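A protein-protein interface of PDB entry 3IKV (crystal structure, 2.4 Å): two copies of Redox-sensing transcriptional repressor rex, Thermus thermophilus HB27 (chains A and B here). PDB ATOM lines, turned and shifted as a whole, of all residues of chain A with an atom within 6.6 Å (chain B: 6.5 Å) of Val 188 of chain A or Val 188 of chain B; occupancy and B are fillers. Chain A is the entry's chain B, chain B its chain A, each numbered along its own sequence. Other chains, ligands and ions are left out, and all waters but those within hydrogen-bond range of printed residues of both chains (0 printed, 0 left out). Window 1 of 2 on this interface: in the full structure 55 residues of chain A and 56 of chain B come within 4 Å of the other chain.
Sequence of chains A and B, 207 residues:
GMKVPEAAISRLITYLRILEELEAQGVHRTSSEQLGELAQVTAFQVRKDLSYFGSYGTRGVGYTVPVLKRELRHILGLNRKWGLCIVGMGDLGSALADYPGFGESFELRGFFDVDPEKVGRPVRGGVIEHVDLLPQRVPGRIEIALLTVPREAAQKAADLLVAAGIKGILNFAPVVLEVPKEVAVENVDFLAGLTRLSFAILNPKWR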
ATOM      1  N   LEU A 170      19.232  21.634 -24.091  1.00  0.00           N
ATOM      2  CA  LEU A 170      17.960  21.115 -24.563  1.00  0.00           C
ATOM      3  C   LEU A 170      18.391  20.086 -25.591  1.00  0.00           C
ATOM      4  O   LEU A 170      18.784  20.437 -26.711  1.00  0.00           O
ATOM      5  CB  LEU A 170      17.149  22.216 -25.232  1.00  0.00           C
ATOM      6  CG  LEU A 170      15.751  21.789 -25.668  1.00  0.00           C
ATOM      7  CD1 LEU A 170      14.985  21.238 -24.457  1.00  0.00           C
ATOM      8  CD2 LEU A 170      15.029  22.983 -26.280  1.00  0.00           C
ATOM      9  N   ASN A 171      18.321  18.817 -25.205  1.00  0.00           N
ATOM     10  CA  ASN A 171      18.769  17.728 -26.065  1.00  0.00           C
ATOM     11  C   ASN A 171      17.732  17.061 -26.971  1.00  0.00           C
ATOM     12  O   ASN A 171      16.716  16.540 -26.502  1.00  0.00           O
ATOM     13  CB  ASN A 171      19.443  16.666 -25.194  1.00  0.00           C
ATOM     14  CG  ASN A 171      19.946  15.503 -25.998  1.00  0.00           C
ATOM     15  OD1 ASN A 171      20.659  15.672 -26.986  1.00  0.00           O
ATOM     16  ND2 ASN A 171      19.580  14.307 -25.582  1.00  0.00           N
ATOM     17  N   PHE A 172      18.015  17.065 -28.274  1.00  0.00           N
ATOM     18  CA  PHE A 172      17.130  16.461 -29.267  1.00  0.00           C
ATOM     19  C   PHE A 172      17.611  15.075 -29.716  1.00  0.00           C
ATOM     20  O   PHE A 172      16.924  14.386 -30.461  1.00  0.00           O
ATOM     21  CB  PHE A 172      16.993  17.379 -30.493  1.00  0.00           C
ATOM     22  CG  PHE A 172      16.199  18.636 -30.233  1.00  0.00           C
ATOM     23  CD1 PHE A 172      16.783  19.731 -29.597  1.00  0.00           C
ATOM     24  CD2 PHE A 172      14.859  18.718 -30.614  1.00  0.00           C
ATOM     25  CE1 PHE A 172      16.043  20.894 -29.343  1.00  0.00           C
ATOM     26  CE2 PHE A 172      14.108  19.873 -30.366  1.00  0.00           C
ATOM     27  CZ  PHE A 172      14.704  20.965 -29.728  1.00  0.00           C
ATOM     28  N   ALA A 173      18.794  14.675 -29.265  1.00  0.00           N
ATOM     29  CA  ALA A 173      19.339  13.373 -29.618  1.00  0.00           C
ATOM     30  C   ALA A 173      18.703  12.300 -28.718  1.00  0.00           C
ATOM     31  O   ALA A 173      18.568  12.500 -27.514  1.00  0.00           O
ATOM     32  CB  ALA A 173      20.860  13.382 -29.445  1.00  0.00           C
ATOM     33  N   PRO A 174      18.307  11.149 -29.299  1.00  0.00           N
ATOM     34  CA  PRO A 174      17.679  10.029 -28.589  1.00  0.00           C
ATOM     35  C   PRO A 174      18.691   9.237 -27.762  1.00  0.00           C
ATOM     36  O   PRO A 174      18.974   8.070 -28.042  1.00  0.00           O
ATOM     37  CB  PRO A 174      17.072   9.217 -29.724  1.00  0.00           C
ATOM     38  CG  PRO A 174      18.094   9.379 -30.797  1.00  0.00           C
ATOM     39  CD  PRO A 174      18.431  10.849 -30.736  1.00  0.00           C
ATOM     40  N   GLU A 186      17.332  18.788 -20.448  1.00  0.00           N
ATOM     41  CA  GLU A 186      15.938  18.523 -20.712  1.00  0.00           C
ATOM     42  C   GLU A 186      15.898  17.872 -22.082  1.00  0.00           C
ATOM     43  O   GLU A 186      16.565  18.334 -23.011  1.00  0.00           O
ATOM     44  CB  GLU A 186      15.141  19.817 -20.712  1.00  0.00           C
ATOM     45  CG  GLU A 186      13.662  19.567 -20.745  1.00  0.00           C
ATOM     46  CD  GLU A 186      13.127  19.041 -19.428  1.00  0.00           C
ATOM     47  OE1 GLU A 186      12.160  18.248 -19.480  1.00  0.00           O
ATOM     48  OE2 GLU A 186      13.656  19.431 -18.354  1.00  0.00           O
ATOM     49  N   ASN A 187      15.127  16.799 -22.219  1.00  0.00           N
ATOM     50  CA  ASN A 187      15.074  16.102 -23.495  1.00  0.00           C
ATOM     51  C   ASN A 187      13.811  16.310 -24.313  1.00  0.00           C
ATOM     52  O   ASN A 187      12.710  16.393 -23.778  1.00  0.00           O
ATOM     53  CB  ASN A 187      15.291  14.594 -23.289  1.00  0.00           C
ATOM     54  CG  ASN A 187      16.717  14.251 -22.848  1.00  0.00           C
ATOM     55  OD1 ASN A 187      17.696  14.714 -23.436  1.00  0.00           O
ATOM     56  ND2 ASN A 187      16.834  13.428 -21.820  1.00  0.00           N
ATOM     57  N   VAL A 188      14.006  16.391 -25.624  1.00  0.00           N
ATOM     58  CA  VAL A 188      12.934  16.555 -26.596  1.00  0.00           C
ATOM     59  C   VAL A 188      13.202  15.430 -27.574  1.00  0.00           C
ATOM     60  O   VAL A 188      13.891  15.597 -28.582  1.00  0.00           O
ATOM     61  CB  VAL A 188      13.026  17.915 -27.322  1.00  0.00           C
ATOM     62  CG1 VAL A 188      12.050  17.951 -28.479  1.00  0.00           C
ATOM     63  CG2 VAL A 188      12.741  19.043 -26.340  1.00  0.00           C
ATOM     64  N   ASP A 189      12.666  14.267 -27.231  1.00  0.00           N
ATOM     65  CA  ASP A 189      12.837  13.039 -27.999  1.00  0.00           C
ATOM     66  C   ASP A 189      11.497  12.681 -28.632  1.00  0.00           C
ATOM     67  O   ASP A 189      10.597  12.187 -27.955  1.00  0.00           O
ATOM     68  CB  ASP A 189      13.290  11.941 -27.026  1.00  0.00           C
ATOM     69  CG  ASP A 189      13.624  10.641 -27.707  1.00  0.00           C
ATOM     70  OD1 ASP A 189      14.155   9.749 -27.018  1.00  0.00           O
ATOM     71  OD2 ASP A 189      13.360  10.500 -28.915  1.00  0.00           O
ATOM     72  N   PHE A 190      11.362  12.922 -29.930  1.00  0.00           N
ATOM     73  CA  PHE A 190      10.096  12.630 -30.586  1.00  0.00           C
ATOM     74  C   PHE A 190       9.950  11.202 -31.074  1.00  0.00           C
ATOM     75  O   PHE A 190       8.843  10.774 -31.362  1.00  0.00           O
ATOM     76  CB  PHE A 190       9.825  13.632 -31.723  1.00  0.00           C
ATOM     77  CG  PHE A 190      10.765  13.525 -32.874  1.00  0.00           C
ATOM     78  CD1 PHE A 190      10.547  12.593 -33.883  1.00  0.00           C
ATOM     79  CD2 PHE A 190      11.854  14.375 -32.966  1.00  0.00           C
ATOM     80  CE1 PHE A 190      11.408  12.510 -34.977  1.00  0.00           C
ATOM     81  CE2 PHE A 190      12.724  14.308 -34.049  1.00  0.00           C
ATOM     82  CZ  PHE A 190      12.502  13.371 -35.061  1.00  0.00           C
ATOM     83  N   LEU A 191      11.054  10.469 -31.185  1.00  0.00           N
ATOM     84  CA  LEU A 191      10.953   9.067 -31.579  1.00  0.00           C
ATOM     85  C   LEU A 191      10.280   8.377 -30.386  1.00  0.00           C
ATOM     86  O   LEU A 191       9.415   7.517 -30.545  1.00  0.00           O
ATOM     87  CB  LEU A 191      12.335   8.453 -31.828  1.00  0.00           C
ATOM     88  CG  LEU A 191      12.850   8.404 -33.272  1.00  0.00           C
ATOM     89  CD1 LEU A 191      14.332   8.023 -33.278  1.00  0.00           C
ATOM     90  CD2 LEU A 191      12.034   7.402 -34.064  1.00  0.00           C
ATOM     91  N   GLY A 193       8.376   9.870 -28.394  1.00  0.00           N
ATOM     92  CA  GLY A 193       7.017  10.374 -28.445  1.00  0.00           C
ATOM     93  C   GLY A 193       6.179   9.560 -29.413  1.00  0.00           C
ATOM     94  O   GLY A 193       5.026   9.232 -29.124  1.00  0.00           O
ATOM     95  N   LEU A 194       6.755   9.247 -30.570  1.00  0.00           N
ATOM     96  CA  LEU A 194       6.066   8.455 -31.581  1.00  0.00           C
ATOM     97  C   LEU A 194       5.779   7.071 -31.036  1.00  0.00           C
ATOM     98  O   LEU A 194       4.712   6.513 -31.275  1.00  0.00           O
ATOM     99  CB  LEU A 194       6.916   8.293 -32.846  1.00  0.00           C
ATOM    100  CG  LEU A 194       6.946   9.377 -33.921  1.00  0.00           C
ATOM    101  CD1 LEU A 194       7.857   8.907 -35.037  1.00  0.00           C
ATOM    102  CD2 LEU A 194       5.537   9.649 -34.459  1.00  0.00           C
ATOM    103  N   LEU B 170       1.020  13.589 -32.874  1.00  0.00           N
ATOM    104  CA  LEU B 170       2.255  13.943 -32.185  1.00  0.00           C
ATOM    105  C   LEU B 170       2.265  15.454 -32.366  1.00  0.00           C
ATOM    106  O   LEU B 170       2.661  15.974 -33.412  1.00  0.00           O
ATOM    107  CB  LEU B 170       3.478  13.305 -32.856  1.00  0.00           C
ATOM    108  CG  LEU B 170       4.823  13.455 -32.122  1.00  0.00           C
ATOM    109  CD1 LEU B 170       4.790  12.700 -30.802  1.00  0.00           C
ATOM    110  CD2 LEU B 170       5.958  12.924 -32.985  1.00  0.00           C
ATOM    111  N   ASN B 171       1.784  16.143 -31.336  1.00  0.00           N
ATOM    112  CA  ASN B 171       1.650  17.594 -31.325  1.00  0.00           C
ATOM    113  C   ASN B 171       2.912  18.370 -30.958  1.00  0.00           C
ATOM    114  O   ASN B 171       3.494  18.176 -29.889  1.00  0.00           O
ATOM    115  CB  ASN B 171       0.503  17.959 -30.376  1.00  0.00           C
ATOM    116  CG  ASN B 171       0.386  19.445 -30.127  1.00  0.00           C
ATOM    117  OD1 ASN B 171       0.465  20.260 -31.052  1.00  0.00           O
ATOM    118  ND2 ASN B 171       0.168  19.810 -28.871  1.00  0.00           N
ATOM    119  N   PHE B 172       3.316  19.260 -31.856  1.00  0.00           N
ATOM    120  CA  PHE B 172       4.497  20.093 -31.646  1.00  0.00           C
ATOM    121  C   PHE B 172       4.116  21.532 -31.272  1.00  0.00           C
ATOM    122  O   PHE B 172       4.973  22.318 -30.873  1.00  0.00           O
ATOM    123  CB  PHE B 172       5.367  20.118 -32.912  1.00  0.00           C
ATOM    124  CG  PHE B 172       6.082  18.826 -33.183  1.00  0.00           C
ATOM    125  CD1 PHE B 172       5.395  17.723 -33.675  1.00  0.00           C
ATOM    126  CD2 PHE B 172       7.444  18.704 -32.920  1.00  0.00           C
ATOM    127  CE1 PHE B 172       6.054  16.514 -33.898  1.00  0.00           C
ATOM    128  CE2 PHE B 172       8.119  17.495 -33.139  1.00  0.00           C
ATOM    129  CZ  PHE B 172       7.422  16.402 -33.630  1.00  0.00           C
ATOM    130  N   ALA B 173       2.836  21.867 -31.403  1.00  0.00           N
ATOM    131  CA  ALA B 173       2.349  23.212 -31.098  1.00  0.00           C
ATOM    132  C   ALA B 173       2.174  23.416 -29.597  1.00  0.00           C
ATOM    133  O   ALA B 173       1.733  22.517 -28.877  1.00  0.00           O
ATOM    134  CB  ALA B 173       1.035  23.470 -31.814  1.00  0.00           C
ATOM    135  N   GLU B 186       0.268  12.932 -28.189  1.00  0.00           N
ATOM    136  CA  GLU B 186       1.544  13.007 -27.495  1.00  0.00           C
ATOM    137  C   GLU B 186       2.112  14.361 -27.842  1.00  0.00           C
ATOM    138  O   GLU B 186       2.116  14.750 -29.009  1.00  0.00           O
ATOM    139  CB  GLU B 186       2.521  11.942 -27.986  1.00  0.00           C
ATOM    140  CG  GLU B 186       2.654  10.736 -27.090  1.00  0.00           C
ATOM    141  CD  GLU B 186       2.924  11.098 -25.651  1.00  0.00           C
ATOM    142  OE1 GLU B 186       3.970  11.716 -25.370  1.00  0.00           O
ATOM    143  OE2 GLU B 186       2.075  10.754 -24.802  1.00  0.00           O
ATOM    144  N   ASN B 187       2.608  15.072 -26.842  1.00  0.00           N
ATOM    145  CA  ASN B 187       3.173  16.392 -27.074  1.00  0.00           C
ATOM    146  C   ASN B 187       4.701  16.394 -27.090  1.00  0.00           C
ATOM    147  O   ASN B 187       5.336  15.788 -26.233  1.00  0.00           O
ATOM    148  CB  ASN B 187       2.678  17.368 -25.993  1.00  0.00           C
ATOM    149  CG  ASN B 187       1.163  17.501 -25.967  1.00  0.00           C
ATOM    150  OD1 ASN B 187       0.557  17.997 -26.913  1.00  0.00           O
ATOM    151  ND2 ASN B 187       0.547  17.057 -24.877  1.00  0.00           N
ATOM    152  N   VAL B 188       5.275  17.063 -28.085  1.00  0.00           N
ATOM    153  CA  VAL B 188       6.718  17.232 -28.208  1.00  0.00           C
ATOM    154  C   VAL B 188       6.825  18.758 -28.165  1.00  0.00           C
ATOM    155  O   VAL B 188       6.812  19.439 -29.197  1.00  0.00           O
ATOM    156  CB  VAL B 188       7.245  16.682 -29.549  1.00  0.00           C
ATOM    157  CG1 VAL B 188       8.754  16.911 -29.657  1.00  0.00           C
ATOM    158  CG2 VAL B 188       6.939  15.206 -29.646  1.00  0.00           C
ATOM    159  N   ASP B 189       6.898  19.273 -26.940  1.00  0.00           N
ATOM    160  CA  ASP B 189       6.927  20.704 -26.634  1.00  0.00           C
ATOM    161  C   ASP B 189       8.322  21.170 -26.263  1.00  0.00           C
ATOM    162  O   ASP B 189       8.696  21.207 -25.094  1.00  0.00           O
ATOM    163  CB  ASP B 189       5.959  20.938 -25.474  1.00  0.00           C
ATOM    164  CG  ASP B 189       5.643  22.388 -25.250  1.00  0.00           C
ATOM    165  OD1 ASP B 189       4.661  22.642 -24.529  1.00  0.00           O
ATOM    166  OD2 ASP B 189       6.363  23.266 -25.767  1.00  0.00           O
ATOM    167  N   PHE B 190       9.081  21.561 -27.272  1.00  0.00           N
ATOM    168  CA  PHE B 190      10.450  21.963 -27.054  1.00  0.00           C
ATOM    169  C   PHE B 190      10.570  23.322 -26.365  1.00  0.00           C
ATOM    170  O   PHE B 190      11.579  23.625 -25.722  1.00  0.00           O
ATOM    171  CB  PHE B 190      11.188  21.947 -28.392  1.00  0.00           C
ATOM    172  CG  PHE B 190      11.214  23.266 -29.063  1.00  0.00           C
ATOM    173  CD1 PHE B 190      10.283  23.602 -30.032  1.00  0.00           C
ATOM    174  CD2 PHE B 190      12.148  24.209 -28.668  1.00  0.00           C
ATOM    175  CE1 PHE B 190      10.287  24.869 -30.595  1.00  0.00           C
ATOM    176  CE2 PHE B 190      12.164  25.466 -29.215  1.00  0.00           C
ATOM    177  CZ  PHE B 190      11.233  25.807 -30.180  1.00  0.00           C
ATOM    178  N   LEU B 191       9.538  24.144 -26.509  1.00  0.00           N
ATOM    179  CA  LEU B 191       9.532  25.462 -25.885  1.00  0.00           C
ATOM    180  C   LEU B 191       9.305  25.283 -24.380  1.00  0.00           C
ATOM    181  O   LEU B 191       9.827  26.042 -23.556  1.00  0.00           O
ATOM    182  CB  LEU B 191       8.433  26.317 -26.502  1.00  0.00           C
ATOM    183  CG  LEU B 191       8.879  27.731 -26.877  1.00  0.00           C
ATOM    184  CD1 LEU B 191       7.929  28.321 -27.894  1.00  0.00           C
ATOM    185  CD2 LEU B 191       8.952  28.585 -25.628  1.00  0.00           C
ATOM    186  N   GLY B 193      10.327  22.682 -22.791  1.00  0.00           N
ATOM    187  CA  GLY B 193      11.574  22.120 -22.293  1.00  0.00           C
ATOM    188  C   GLY B 193      12.538  23.253 -22.030  1.00  0.00           C
ATOM    189  O   GLY B 193      13.296  23.260 -21.057  1.00  0.00           O
ATOM    190  N   LEU B 194      12.478  24.238 -22.916  1.00  0.00           N
ATOM    191  CA  LEU B 194      13.309  25.423 -22.828  1.00  0.00           C
ATOM    192  C   LEU B 194      12.950  26.140 -21.528  1.00  0.00           C
ATOM    193  O   LEU B 194      13.819  26.568 -20.772  1.00  0.00           O
ATOM    194  CB  LEU B 194      13.018  26.302 -24.034  1.00  0.00           C
ATOM    195  CG  LEU B 194      14.082  27.248 -24.562  1.00  0.00           C
ATOM    196  CD1 LEU B 194      15.455  26.591 -24.495  1.00  0.00           C
ATOM    197  CD2 LEU B 194      13.730  27.613 -26.006  1.00  0.00           C
ATOM    198  N   ARG B 196      11.512  24.721 -18.991  1.00  0.00           N
ATOM    199  CA  ARG B 196      11.846  23.830 -17.882  1.00  0.00           C
ATOM    200  C   ARG B 196      13.324  24.029 -17.515  1.00  0.00           C
ATOM    201  O   ARG B 196      13.705  23.944 -16.342  1.00  0.00           O
ATOM    202  CB  ARG B 196      11.569  22.364 -18.249  1.00  0.00           C
ATOM    203  CG  ARG B 196      10.114  21.961 -18.096  1.00  0.00           C
ATOM    204  CD  ARG B 196       9.931  20.452 -18.197  1.00  0.00           C
ATOM    205  NE  ARG B 196       9.916  19.964 -19.571  1.00  0.00           N
ATOM    206  CZ  ARG B 196       8.832  19.926 -20.341  1.00  0.00           C
ATOM    207  NH1 ARG B 196       7.662  20.343 -19.867  1.00  0.00           N
ATOM    208  NH2 ARG B 196       8.918  19.478 -21.590  1.00  0.00           N
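Leu 170 of chain A touches Phe 190 of chain B.
Leu 170 of chain A touches Gly 193 of chain B (CD1 to C, 3.99 Å).
Phe 190 of chain B touches Phe 172 of chain A.
Glu 186 of chain A touches Gly 193 of chain B.
CG1 of Val 188 of chain B touches CG1 of Val 188 of chain A (3.7 Å).
CG2 of Val 188 of chain A touches CA of Phe 190 of chain B (3.8 Å).
O of Phe 190 of chain A touches CD2 of Leu 170 of chain B (3.9 Å).
Phe 190 of chain A touches Val 188 of chain B.
CG of Glu 186 of chain B touches O of Gly 193 of chain A, at 3.5 Å.
CD2 of Leu 194 of chain A touches CD2 of Leu 170 of chain B, at 3.6 Å.
Leu 170 of chain A touches Phe 190 of chain B, and with the chains exchanged Phe 190 of chain A touches Leu 170 of chain B.
Leu 170 of chain A touches Gly 193 of chain B, and with the chains exchanged Gly 193 of chain A touches Leu 170 of chain B.
Val 188 of chain B touches its own counterpart, Val 188 of chain A.
Leu 194 of chain A touches Leu 170 of chain B, but with the chains exchanged Leu 170 of chain A does not touch Leu 194 of chain B (4.05 Å).
Of the 12 pairs that touch across the chains among the printed residues, 9 have their exchanged pair printed and touching as well.
Of the printed residues of chain B, Phe 172 of chain A touches Phe 190 (3.9 Å).
Val 188 of chain A touches just these residues of chain B: Val 188 and Phe 190.
Val 188 of chain B touches two residues of chain A.
Printed residues of chain A within 4 Å of Phe 190 of chain B: Leu 170, Phe 172 and Val 188.
Of the printed residues of chain A, Arg 196 of chain B touches Glu 186 (2.8 Å).
The backbone NH (N) of Asn 171 of chain B lies within hydrogen-bond range of the backbone carbonyl oxygen (O) of Glu 186 of chain B (2.7 Å).
The backbone carbonyl oxygen (O) of Asn 171 of chain B lies within hydrogen-bond range of the backbone NH (N) of Val 188 of chain B (2.8 Å).
N of Asn 171 of chain A sits at hydrogen-bond distance from O of Glu 186 of chain A (2.9 Å).
The backbone carbonyl oxygen of Asn 171 of chain A lies within hydrogen-bond range of the backbone NH of Val 188 of chain A (2.9 Å).
Of the 13 printed residues of chain B, 6 touch a printed residue of chain A.
Printed residues of chain B that touch a printed residue of chain A: Leu 170, Glu 186, Val 188, Phe 190, Gly 193 and Arg 196.
Hydrophobic or aromatic side chains of chain B within 4 Å of the printed part of chain A: Leu 170, Val 188 and Phe 190.
Hydrophobic or aromatic side chains of chain A that line the printed part of chain B: Leu 170, Phe 172, Val 188, Phe 190 and Leu 194.
NE of Arg 196 of chain B lies within salt-bridge range of OE1 of Glu 186 of chain A (2.8 Å).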
